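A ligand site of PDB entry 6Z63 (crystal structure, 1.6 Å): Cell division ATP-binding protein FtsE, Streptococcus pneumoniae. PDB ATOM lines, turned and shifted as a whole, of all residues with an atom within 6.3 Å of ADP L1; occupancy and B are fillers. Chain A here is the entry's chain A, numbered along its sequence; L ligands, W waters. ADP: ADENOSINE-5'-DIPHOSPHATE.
N of Thr 45 is in hydrogen-bond range of O1A of ADP L1, 3.0 Å away.
An oxygen (O1A) of ADP L1 sits at hydrogen-bond distance from the side-chain hydroxyl of Thr 45, 2.6 Å away.
An oxygen (O1B) of ADP L1 lies within hydrogen-bond range of the backbone NH of Lys 43, at 2.9 Å.
O1B of ADP L1 is in salt-bridge range of NZ of Lys 43.
An oxygen (O3B) of ADP L1 is in hydrogen-bond range of the backbone NH (N) of Ser 44.
OG of Ser 44 is in hydrogen-bond range of O3B of ADP L1, at 2.9 Å.
O2B of ADP L1 sits at hydrogen-bond distance from N of Gly 40, at 2.8 Å.
O1B of ADP L1 is in hydrogen-bond range of N of Gly 42, 2.9 Å away.
The backbone NH of Ala 41 lies within hydrogen-bond range of an oxygen (O1B) of ADP L1, at 3.1 Å.
The side-chain hydroxyl (OH) of Tyr 13 sits at hydrogen-bond distance from the side-chain hydroxyl (OG1) of Thr 45 (2.6 Å).
NZ of Lys 43 lies within hydrogen-bond range of O of Pro 38 (3.0 Å).
The side-chain amino group (NZ) of Lys 43 lies within hydrogen-bond range of the backbone carbonyl oxygen (O) of Gly 37, at 2.9 Å.
NZ of Lys 43 sits at hydrogen-bond distance from NE2 of His 197, 3.5 Å away.
The side-chain hydroxyl (OG) of Ser 44 lies within hydrogen-bond range of the side-chain carboxylate (OD2) of Asp 164, 3.4 Å away.
The side-chain amide oxygen (OD1) of Asn 15 lies within hydrogen-bond range of the backbone NH (N) of Thr 17 (3.0 Å).
CD2 of Tyr 13 touches C4 of ADP L1 (3.4 Å).
Asn 15 touches ADP L1 (OD1 to C2, 3.7 Å).
Thr 17 touches ADP L1.
Ala 19 touches ADP L1.
O of Pro 38 touches O1B of ADP L1, at 3.6 Å.
Ser 39 touches ADP L1.
12 residues have an atom within 4 Å of ADP L1: Tyr 13, Asn 15, Thr 17, Ala 19, Pro 38, Ser 39, Gly 40, Ala 41, Gly 42, Lys 43, Ser 44 and Thr 45.
The nearest printed residue that does not touch ADP L1 is Arg 48 (4.6 Å).
Water W8 lies within hydrogen-bond range of O2B of ADP L1 (2.5 Å), NE2 of His 197 (3.0 Å) and NZ of Lys 43 (3.1 Å).
Water W5 lies within hydrogen-bond range of an oxygen (O2') of ADP L1 (2.6 Å) and a nitrogen (N1) of ADP L2 (2.9 Å).
Water W2 lies within hydrogen-bond range of OG1 of Thr 17 (2.6 Å), N3 of ADP L1 (2.7 Å) and ND2 of Asn 15 (2.9 Å).
Water W1 lies within hydrogen-bond range of O2A of ADP L1 (2.8 Å) and NH2 of Arg 48 (2.8 Å).
Water W4 bridges a nitrogen (N7) of ADP L1 and the guanidinium group (NH2) of Arg 48.
Water W6 bridges a nitrogen (N1) of ADP L1 (3.1 Å) and the backbone NH (N) of Asn 15 (3.1 Å).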
ATOM      1  N   TYR A  13      21.950  20.453 -31.020  1.00  0.00           N
ATOM      2  CA  TYR A  13      21.230  19.315 -31.576  1.00  0.00           C
ATOM      3  C   TYR A  13      21.929  18.814 -32.849  1.00  0.00           C
ATOM      4  O   TYR A  13      22.820  19.458 -33.402  1.00  0.00           O
ATOM      5  CB  TYR A  13      19.768  19.678 -31.844  1.00  0.00           C
ATOM      6  CG  TYR A  13      18.950  19.772 -30.567  1.00  0.00           C
ATOM      7  CD1 TYR A  13      18.573  18.635 -29.880  1.00  0.00           C
ATOM      8  CD2 TYR A  13      18.581  21.009 -30.054  1.00  0.00           C
ATOM      9  CE1 TYR A  13      17.842  18.707 -28.706  1.00  0.00           C
ATOM     10  CE2 TYR A  13      17.834  21.088 -28.881  1.00  0.00           C
ATOM     11  CZ  TYR A  13      17.464  19.935 -28.221  1.00  0.00           C
ATOM     12  OH  TYR A  13      16.737  19.960 -27.039  1.00  0.00           O
ATOM     13  N   ASP A  14      21.498  17.634 -33.309  1.00  0.00           N
ATOM     14  CA  ASP A  14      22.187  16.995 -34.425  1.00  0.00           C
ATOM     15  C   ASP A  14      22.152  17.845 -35.694  1.00  0.00           C
ATOM     16  O   ASP A  14      23.072  17.779 -36.509  1.00  0.00           O
ATOM     17  CB  ASP A  14      21.583  15.619 -34.713  1.00  0.00           C
ATOM     18  CG  ASP A  14      22.048  14.558 -33.728  1.00  0.00           C
ATOM     19  OD1 ASP A  14      23.115  14.751 -33.092  1.00  0.00           O
ATOM     20  OD2 ASP A  14      21.356  13.525 -33.591  1.00  0.00           O
ATOM     21  N   ASN A  15      21.093  18.639 -35.888  1.00  0.00           N
ATOM     22  CA  ASN A  15      21.014  19.477 -37.070  1.00  0.00           C
ATOM     23  C   ASN A  15      21.836  20.755 -36.964  1.00  0.00           C
ATOM     24  O   ASN A  15      21.811  21.575 -37.893  1.00  0.00           O
ATOM     25  CB  ASN A  15      19.560  19.821 -37.379  1.00  0.00           C
ATOM     26  CG  ASN A  15      19.006  20.910 -36.474  1.00  0.00           C
ATOM     27  OD1 ASN A  15      19.607  21.233 -35.450  1.00  0.00           O
ATOM     28  ND2 ASN A  15      17.883  21.493 -36.857  1.00  0.00           N
ATOM     29  N   THR A  17      21.615  23.219 -34.493  1.00  0.00           N
ATOM     30  CA  THR A  17      21.054  24.288 -33.685  1.00  0.00           C
ATOM     31  C   THR A  17      21.614  24.240 -32.268  1.00  0.00           C
ATOM     32  O   THR A  17      21.512  23.211 -31.588  1.00  0.00           O
ATOM     33  CB  THR A  17      19.542  24.168 -33.650  1.00  0.00           C
ATOM     34  OG1 THR A  17      19.029  24.324 -34.983  1.00  0.00           O
ATOM     35  CG2 THR A  17      18.928  25.204 -32.738  1.00  0.00           C
ATOM     36  N   THR A  18      22.227  25.331 -31.806  1.00  0.00           N
ATOM     37  CA  THR A  18      22.790  25.368 -30.452  1.00  0.00           C
ATOM     38  C   THR A  18      21.731  25.920 -29.514  1.00  0.00           C
ATOM     39  O   THR A  18      21.502  27.134 -29.468  1.00  0.00           O
ATOM     40  CB  THR A  18      24.080  26.186 -30.397  1.00  0.00           C
ATOM     41  OG1 THR A  18      24.981  25.732 -31.418  1.00  0.00           O
ATOM     42  CG2 THR A  18      24.739  26.006 -29.030  1.00  0.00           C
ATOM     43  N   ALA A  19      21.120  25.034 -28.719  1.00  0.00           N
ATOM     44  CA  ALA A  19      19.968  25.356 -27.882  1.00  0.00           C
ATOM     45  C   ALA A  19      20.353  25.928 -26.520  1.00  0.00           C
ATOM     46  O   ALA A  19      19.605  26.749 -25.970  1.00  0.00           O
ATOM     47  CB  ALA A  19      19.100  24.115 -27.694  1.00  0.00           C
ATOM     48  N   LEU A  20      21.466  25.489 -25.930  1.00  0.00           N
ATOM     49  CA  LEU A  20      22.012  26.086 -24.713  1.00  0.00           C
ATOM     50  C   LEU A  20      23.433  26.500 -25.016  1.00  0.00           C
ATOM     51  O   LEU A  20      24.208  25.713 -25.557  1.00  0.00           O
ATOM     52  CB  LEU A  20      21.987  25.110 -23.532  1.00  0.00           C
ATOM     53  CG  LEU A  20      20.608  24.555 -23.170  1.00  0.00           C
ATOM     54  CD1 LEU A  20      20.700  23.553 -22.020  1.00  0.00           C
ATOM     55  CD2 LEU A  20      19.699  25.700 -22.801  1.00  0.00           C
ATOM     56  N   GLY A  37      11.096  32.494 -20.421  1.00  0.00           N
ATOM     57  CA  GLY A  37      11.739  33.017 -21.617  1.00  0.00           C
ATOM     58  C   GLY A  37      10.947  32.788 -22.887  1.00  0.00           C
ATOM     59  O   GLY A  37       9.994  31.996 -22.912  1.00  0.00           O
ATOM     60  N   PRO A  38      11.328  33.453 -23.979  1.00  0.00           N
ATOM     61  CA  PRO A  38      10.552  33.338 -25.224  1.00  0.00           C
ATOM     62  C   PRO A  38      10.628  31.936 -25.807  1.00  0.00           C
ATOM     63  O   PRO A  38      11.464  31.110 -25.433  1.00  0.00           O
ATOM     64  CB  PRO A  38      11.225  34.354 -26.166  1.00  0.00           C
ATOM     65  CG  PRO A  38      12.128  35.186 -25.303  1.00  0.00           C
ATOM     66  CD  PRO A  38      12.482  34.358 -24.111  1.00  0.00           C
ATOM     67  N   SER A  39       9.714  31.664 -26.736  1.00  0.00           N
ATOM     68  CA  SER A  39       9.789  30.453 -27.528  1.00  0.00           C
ATOM     69  C   SER A  39      11.184  30.305 -28.103  1.00  0.00           C
ATOM     70  O   SER A  39      11.753  31.256 -28.650  1.00  0.00           O
ATOM     71  CB  SER A  39       8.758  30.484 -28.670  1.00  0.00           C
ATOM     72  OG  SER A  39       7.444  30.247 -28.192  1.00  0.00           O
ATOM     73  N   GLY A  40      11.725  29.098 -27.995  1.00  0.00           N
ATOM     74  CA  GLY A  40      13.022  28.785 -28.552  1.00  0.00           C
ATOM     75  C   GLY A  40      14.211  29.210 -27.715  1.00  0.00           C
ATOM     76  O   GLY A  40      15.336  29.043 -28.169  1.00  0.00           O
ATOM     77  N   ALA A  41      13.984  29.751 -26.514  1.00  0.00           N
ATOM     78  CA  ALA A  41      15.100  30.181 -25.679  1.00  0.00           C
ATOM     79  C   ALA A  41      15.929  29.011 -25.186  1.00  0.00           C
ATOM     80  O   ALA A  41      17.130  29.165 -24.923  1.00  0.00           O
ATOM     81  CB  ALA A  41      14.591  31.000 -24.495  1.00  0.00           C
ATOM     82  N   GLY A  42      15.297  27.843 -25.021  1.00  0.00           N
ATOM     83  CA  GLY A  42      15.982  26.652 -24.578  1.00  0.00           C
ATOM     84  C   GLY A  42      15.437  26.115 -23.271  1.00  0.00           C
ATOM     85  O   GLY A  42      16.088  25.303 -22.629  1.00  0.00           O
ATOM     86  N   LYS A  43      14.249  26.577 -22.871  1.00  0.00           N
ATOM     87  CA  LYS A  43      13.658  26.130 -21.614  1.00  0.00           C
ATOM     88  C   LYS A  43      13.470  24.610 -21.575  1.00  0.00           C
ATOM     89  O   LYS A  43      13.783  23.961 -20.569  1.00  0.00           O
ATOM     90  CB  LYS A  43      12.323  26.836 -21.376  1.00  0.00           C
ATOM     91  CG  LYS A  43      12.441  28.348 -21.200  1.00  0.00           C
ATOM     92  CD  LYS A  43      11.068  28.982 -20.951  1.00  0.00           C
ATOM     93  CE  LYS A  43      10.053  28.622 -22.039  1.00  0.00           C
ATOM     94  NZ  LYS A  43      10.374  29.154 -23.413  1.00  0.00           N
ATOM     95  N   SER A  44      12.893  24.045 -22.633  1.00  0.00           N
ATOM     96  CA  SER A  44      12.602  22.615 -22.630  1.00  0.00           C
ATOM     97  C   SER A  44      13.887  21.809 -22.632  1.00  0.00           C
ATOM     98  O   SER A  44      13.972  20.775 -21.963  1.00  0.00           O
ATOM     99  CB  SER A  44      11.759  22.224 -23.840  1.00  0.00           C
ATOM    100  OG  SER A  44      10.465  22.801 -23.774  1.00  0.00           O
ATOM    101  N   THR A  45      14.889  22.278 -23.393  1.00  0.00           N
ATOM    102  CA  THR A  45      16.184  21.608 -23.416  1.00  0.00           C
ATOM    103  C   THR A  45      16.830  21.607 -22.033  1.00  0.00           C
ATOM    104  O   THR A  45      17.347  20.584 -21.575  1.00  0.00           O
ATOM    105  CB  THR A  45      17.092  22.278 -24.438  1.00  0.00           C
ATOM    106  OG1 THR A  45      16.487  22.201 -25.736  1.00  0.00           O
ATOM    107  CG2 THR A  45      18.459  21.581 -24.484  1.00  0.00           C
ATOM    108  N   PHE A  46      16.770  22.758 -21.361  1.00  0.00           N
ATOM    109  CA  PHE A  46      17.272  22.860 -19.989  1.00  0.00           C
ATOM    110  C   PHE A  46      16.554  21.901 -19.041  1.00  0.00           C
ATOM    111  O   PHE A  46      17.198  21.152 -18.294  1.00  0.00           O
ATOM    112  CB  PHE A  46      17.117  24.318 -19.536  1.00  0.00           C
ATOM    113  CG  PHE A  46      17.356  24.540 -18.087  1.00  0.00           C
ATOM    114  CD1 PHE A  46      18.631  24.829 -17.635  1.00  0.00           C
ATOM    115  CD2 PHE A  46      16.333  24.459 -17.178  1.00  0.00           C
ATOM    116  CE1 PHE A  46      18.872  25.036 -16.283  1.00  0.00           C
ATOM    117  CE2 PHE A  46      16.565  24.659 -15.840  1.00  0.00           C
ATOM    118  CZ  PHE A  46      17.832  24.942 -15.388  1.00  0.00           C
ATOM    119  N   ARG A  48      14.894  19.150 -19.732  1.00  0.00           N
ATOM    120  CA  ARG A  48      15.179  17.761 -20.086  1.00  0.00           C
ATOM    121  C   ARG A  48      16.581  17.363 -19.663  1.00  0.00           C
ATOM    122  O   ARG A  48      16.804  16.188 -19.342  1.00  0.00           O
ATOM    123  CB  ARG A  48      14.986  17.534 -21.585  1.00  0.00           C
ATOM    124  CG  ARG A  48      13.523  17.601 -22.022  1.00  0.00           C
ATOM    125  CD  ARG A  48      13.405  17.675 -23.545  1.00  0.00           C
ATOM    126  NE  ARG A  48      12.066  18.083 -23.990  1.00  0.00           N
ATOM    127  CZ  ARG A  48      11.809  18.822 -25.066  1.00  0.00           C
ATOM    128  NH1 ARG A  48      10.563  19.148 -25.390  1.00  0.00           N
ATOM    129  NH2 ARG A  48      12.814  19.266 -25.831  1.00  0.00           N
ATOM    130  N   ASP A 164       7.622  20.711 -16.747  1.00  0.00           N
ATOM    131  CA  ASP A 164       7.684  21.481 -17.996  1.00  0.00           C
ATOM    132  C   ASP A 164       6.273  21.962 -18.339  1.00  0.00           C
ATOM    133  O   ASP A 164       5.445  21.176 -18.793  1.00  0.00           O
ATOM    134  CB  ASP A 164       8.263  20.632 -19.116  1.00  0.00           C
ATOM    135  CG  ASP A 164       8.704  21.455 -20.326  1.00  0.00           C
ATOM    136  OD1 ASP A 164       8.527  22.693 -20.326  1.00  0.00           O
ATOM    137  OD2 ASP A 164       9.199  20.846 -21.299  1.00  0.00           O
ATOM    138  N   GLU A 165       6.009  23.259 -18.114  1.00  0.00           N
ATOM    139  CA  GLU A 165       4.689  23.843 -18.321  1.00  0.00           C
ATOM    140  C   GLU A 165       3.573  22.995 -17.718  1.00  0.00           C
ATOM    141  O   GLU A 165       2.636  22.594 -18.426  1.00  0.00           O
ATOM    142  CB  GLU A 165       4.419  24.098 -19.802  1.00  0.00           C
ATOM    143  CG  GLU A 165       5.460  24.965 -20.474  1.00  0.00           C
ATOM    144  CD  GLU A 165       4.909  25.649 -21.703  1.00  0.00           C
ATOM    145  OE1 GLU A 165       3.775  26.190 -21.644  1.00  0.00           O
ATOM    146  OE2 GLU A 165       5.613  25.642 -22.738  1.00  0.00           O
ATOM    147  N   HIS A 197       5.017  29.555 -19.257  1.00  0.00           N
ATOM    148  CA  HIS A 197       4.676  30.775 -19.987  1.00  0.00           C
ATOM    149  C   HIS A 197       3.574  31.562 -19.300  1.00  0.00           C
ATOM    150  O   HIS A 197       3.087  32.559 -19.876  1.00  0.00           O
ATOM    151  CB  HIS A 197       4.235  30.425 -21.413  1.00  0.00           C
ATOM    152  CG  HIS A 197       5.367  30.144 -22.342  1.00  0.00           C
ATOM    153  ND1 HIS A 197       6.168  31.139 -22.865  1.00  0.00           N
ATOM    154  CD2 HIS A 197       5.851  28.972 -22.827  1.00  0.00           C
ATOM    155  CE1 HIS A 197       7.092  30.582 -23.633  1.00  0.00           C
ATOM    156  NE2 HIS A 197       6.912  29.279 -23.627  1.00  0.00           N
HETATM  157  PB  ADP L   1      11.831  26.526 -25.506  1.00  0.00           P
HETATM  158  O1B ADP L   1      12.374  27.713 -24.752  1.00  0.00           O
HETATM  159  O2B ADP L   1      10.781  26.901 -26.515  1.00  0.00           O
HETATM  160  O3B ADP L   1      11.405  25.405 -24.587  1.00  0.00           O
HETATM  161  PA  ADP L   1      13.501  24.453 -26.774  1.00  0.00           P
HETATM  162  O1A ADP L   1      14.515  23.958 -25.797  1.00  0.00           O
HETATM  163  O2A ADP L   1      12.273  23.644 -27.001  1.00  0.00           O
HETATM  164  O3A ADP L   1      13.079  25.943 -26.359  1.00  0.00           O
HETATM  165  O5' ADP L   1      14.222  24.720 -28.187  1.00  0.00           O
HETATM  166  C5' ADP L   1      15.471  25.461 -28.200  1.00  0.00           C
HETATM  167  C4' ADP L   1      15.928  25.640 -29.624  1.00  0.00           C
HETATM  168  O4' ADP L   1      16.377  24.367 -30.144  1.00  0.00           O
HETATM  169  C3' ADP L   1      14.861  26.125 -30.621  1.00  0.00           C
HETATM  170  O3' ADP L   1      15.433  26.886 -31.676  1.00  0.00           O
HETATM  171  C2' ADP L   1      14.282  24.796 -31.132  1.00  0.00           C
HETATM  172  O2' ADP L   1      13.691  24.915 -32.403  1.00  0.00           O
HETATM  173  C1' ADP L   1      15.543  23.924 -31.188  1.00  0.00           C
HETATM  174  N9  ADP L   1      15.281  22.508 -31.001  1.00  0.00           N
HETATM  175  C8  ADP L   1      14.523  21.932 -30.013  1.00  0.00           C
HETATM  176  N7  ADP L   1      14.464  20.631 -30.085  1.00  0.00           N
HETATM  177  C5  ADP L   1      15.217  20.314 -31.207  1.00  0.00           C
HETATM  178  C6  ADP L   1      15.545  19.094 -31.815  1.00  0.00           C
HETATM  179  N6  ADP L   1      15.118  17.912 -31.373  1.00  0.00           N
HETATM  180  N1  ADP L   1      16.324  19.129 -32.920  1.00  0.00           N
HETATM  181  C2  ADP L   1      16.747  20.319 -33.356  1.00  0.00           C
HETATM  182  N3  ADP L   1      16.508  21.531 -32.867  1.00  0.00           N
HETATM  183  C4  ADP L   1      15.732  21.470 -31.779  1.00  0.00           C
HETATM  184  PB  ADP L   2      12.630  10.486 -34.500  1.00  0.00           P
HETATM  185  O1B ADP L   2      13.694   9.436 -34.703  1.00  0.00           O
HETATM  186  O2B ADP L   2      11.909  10.843 -35.767  1.00  0.00           O
HETATM  187  O3B ADP L   2      11.691  10.157 -33.367  1.00  0.00           O
HETATM  188  PA  ADP L   2      13.221  13.368 -34.394  1.00  0.00           P
HETATM  189  O1A ADP L   2      14.545  14.062 -34.256  1.00  0.00           O
HETATM  190  O2A ADP L   2      12.506  13.475 -35.694  1.00  0.00           O
HETATM  191  O3A ADP L   2      13.420  11.826 -34.039  1.00  0.00           O
HETATM  192  O5' ADP L   2      12.255  13.834 -33.212  1.00  0.00           O
HETATM  193  C5' ADP L   2      11.024  14.525 -33.557  1.00  0.00           C
HETATM  194  C4' ADP L   2      10.721  15.564 -32.505  1.00  0.00           C
HETATM  195  O4' ADP L   2      11.956  16.227 -32.119  1.00  0.00           O
HETATM  196  C3' ADP L   2       9.764  16.686 -32.920  1.00  0.00           C
HETATM  197  O3' ADP L   2       8.411  16.352 -32.635  1.00  0.00           O
HETATM  198  C2' ADP L   2      10.251  17.863 -32.072  1.00  0.00           C
HETATM  199  O2' ADP L   2       9.733  17.829 -30.757  1.00  0.00           O
HETATM  200  C1' ADP L   2      11.757  17.624 -32.088  1.00  0.00           C
HETATM  201  N9  ADP L   2      12.433  18.217 -33.230  1.00  0.00           N
HETATM  202  C8  ADP L   2      13.028  17.549 -34.271  1.00  0.00           C
HETATM  203  N7  ADP L   2      13.561  18.338 -35.166  1.00  0.00           N
HETATM  204  C5  ADP L   2      13.306  19.613 -34.694  1.00  0.00           C
HETATM  205  C6  ADP L   2      13.627  20.888 -35.194  1.00  0.00           C
HETATM  206  N6  ADP L   2      14.288  21.097 -36.327  1.00  0.00           N
HETATM  207  N1  ADP L   2      13.220  21.960 -34.478  1.00  0.00           N
HETATM  208  C2  ADP L   2      12.551  21.748 -33.330  1.00  0.00           C
HETATM  209  N3  ADP L   2      12.205  20.602 -32.764  1.00  0.00           N
HETATM  210  C4  ADP L   2      12.614  19.562 -33.500  1.00  0.00           C
HETATM  211  O   HOH W   1      11.912  21.026 -27.825  1.00  0.00           O
HETATM  212  O   HOH W   2      16.678  23.270 -34.886  1.00  0.00           O
HETATM  213  O   HOH W   3      11.190  23.507 -30.522  1.00  0.00           O
HETATM  214  O   HOH W   4      13.305  18.101 -28.828  1.00  0.00           O
HETATM  215  O   HOH W   5      14.329  24.584 -34.927  1.00  0.00           O
HETATM  216  O   HOH W   6      18.303  17.785 -34.819  1.00  0.00           O
HETATM  217  O   HOH W   7      18.122  28.365 -30.783  1.00  0.00           O
HETATM  218  O   HOH W   8       8.602  27.532 -25.431  1.00  0.00           O
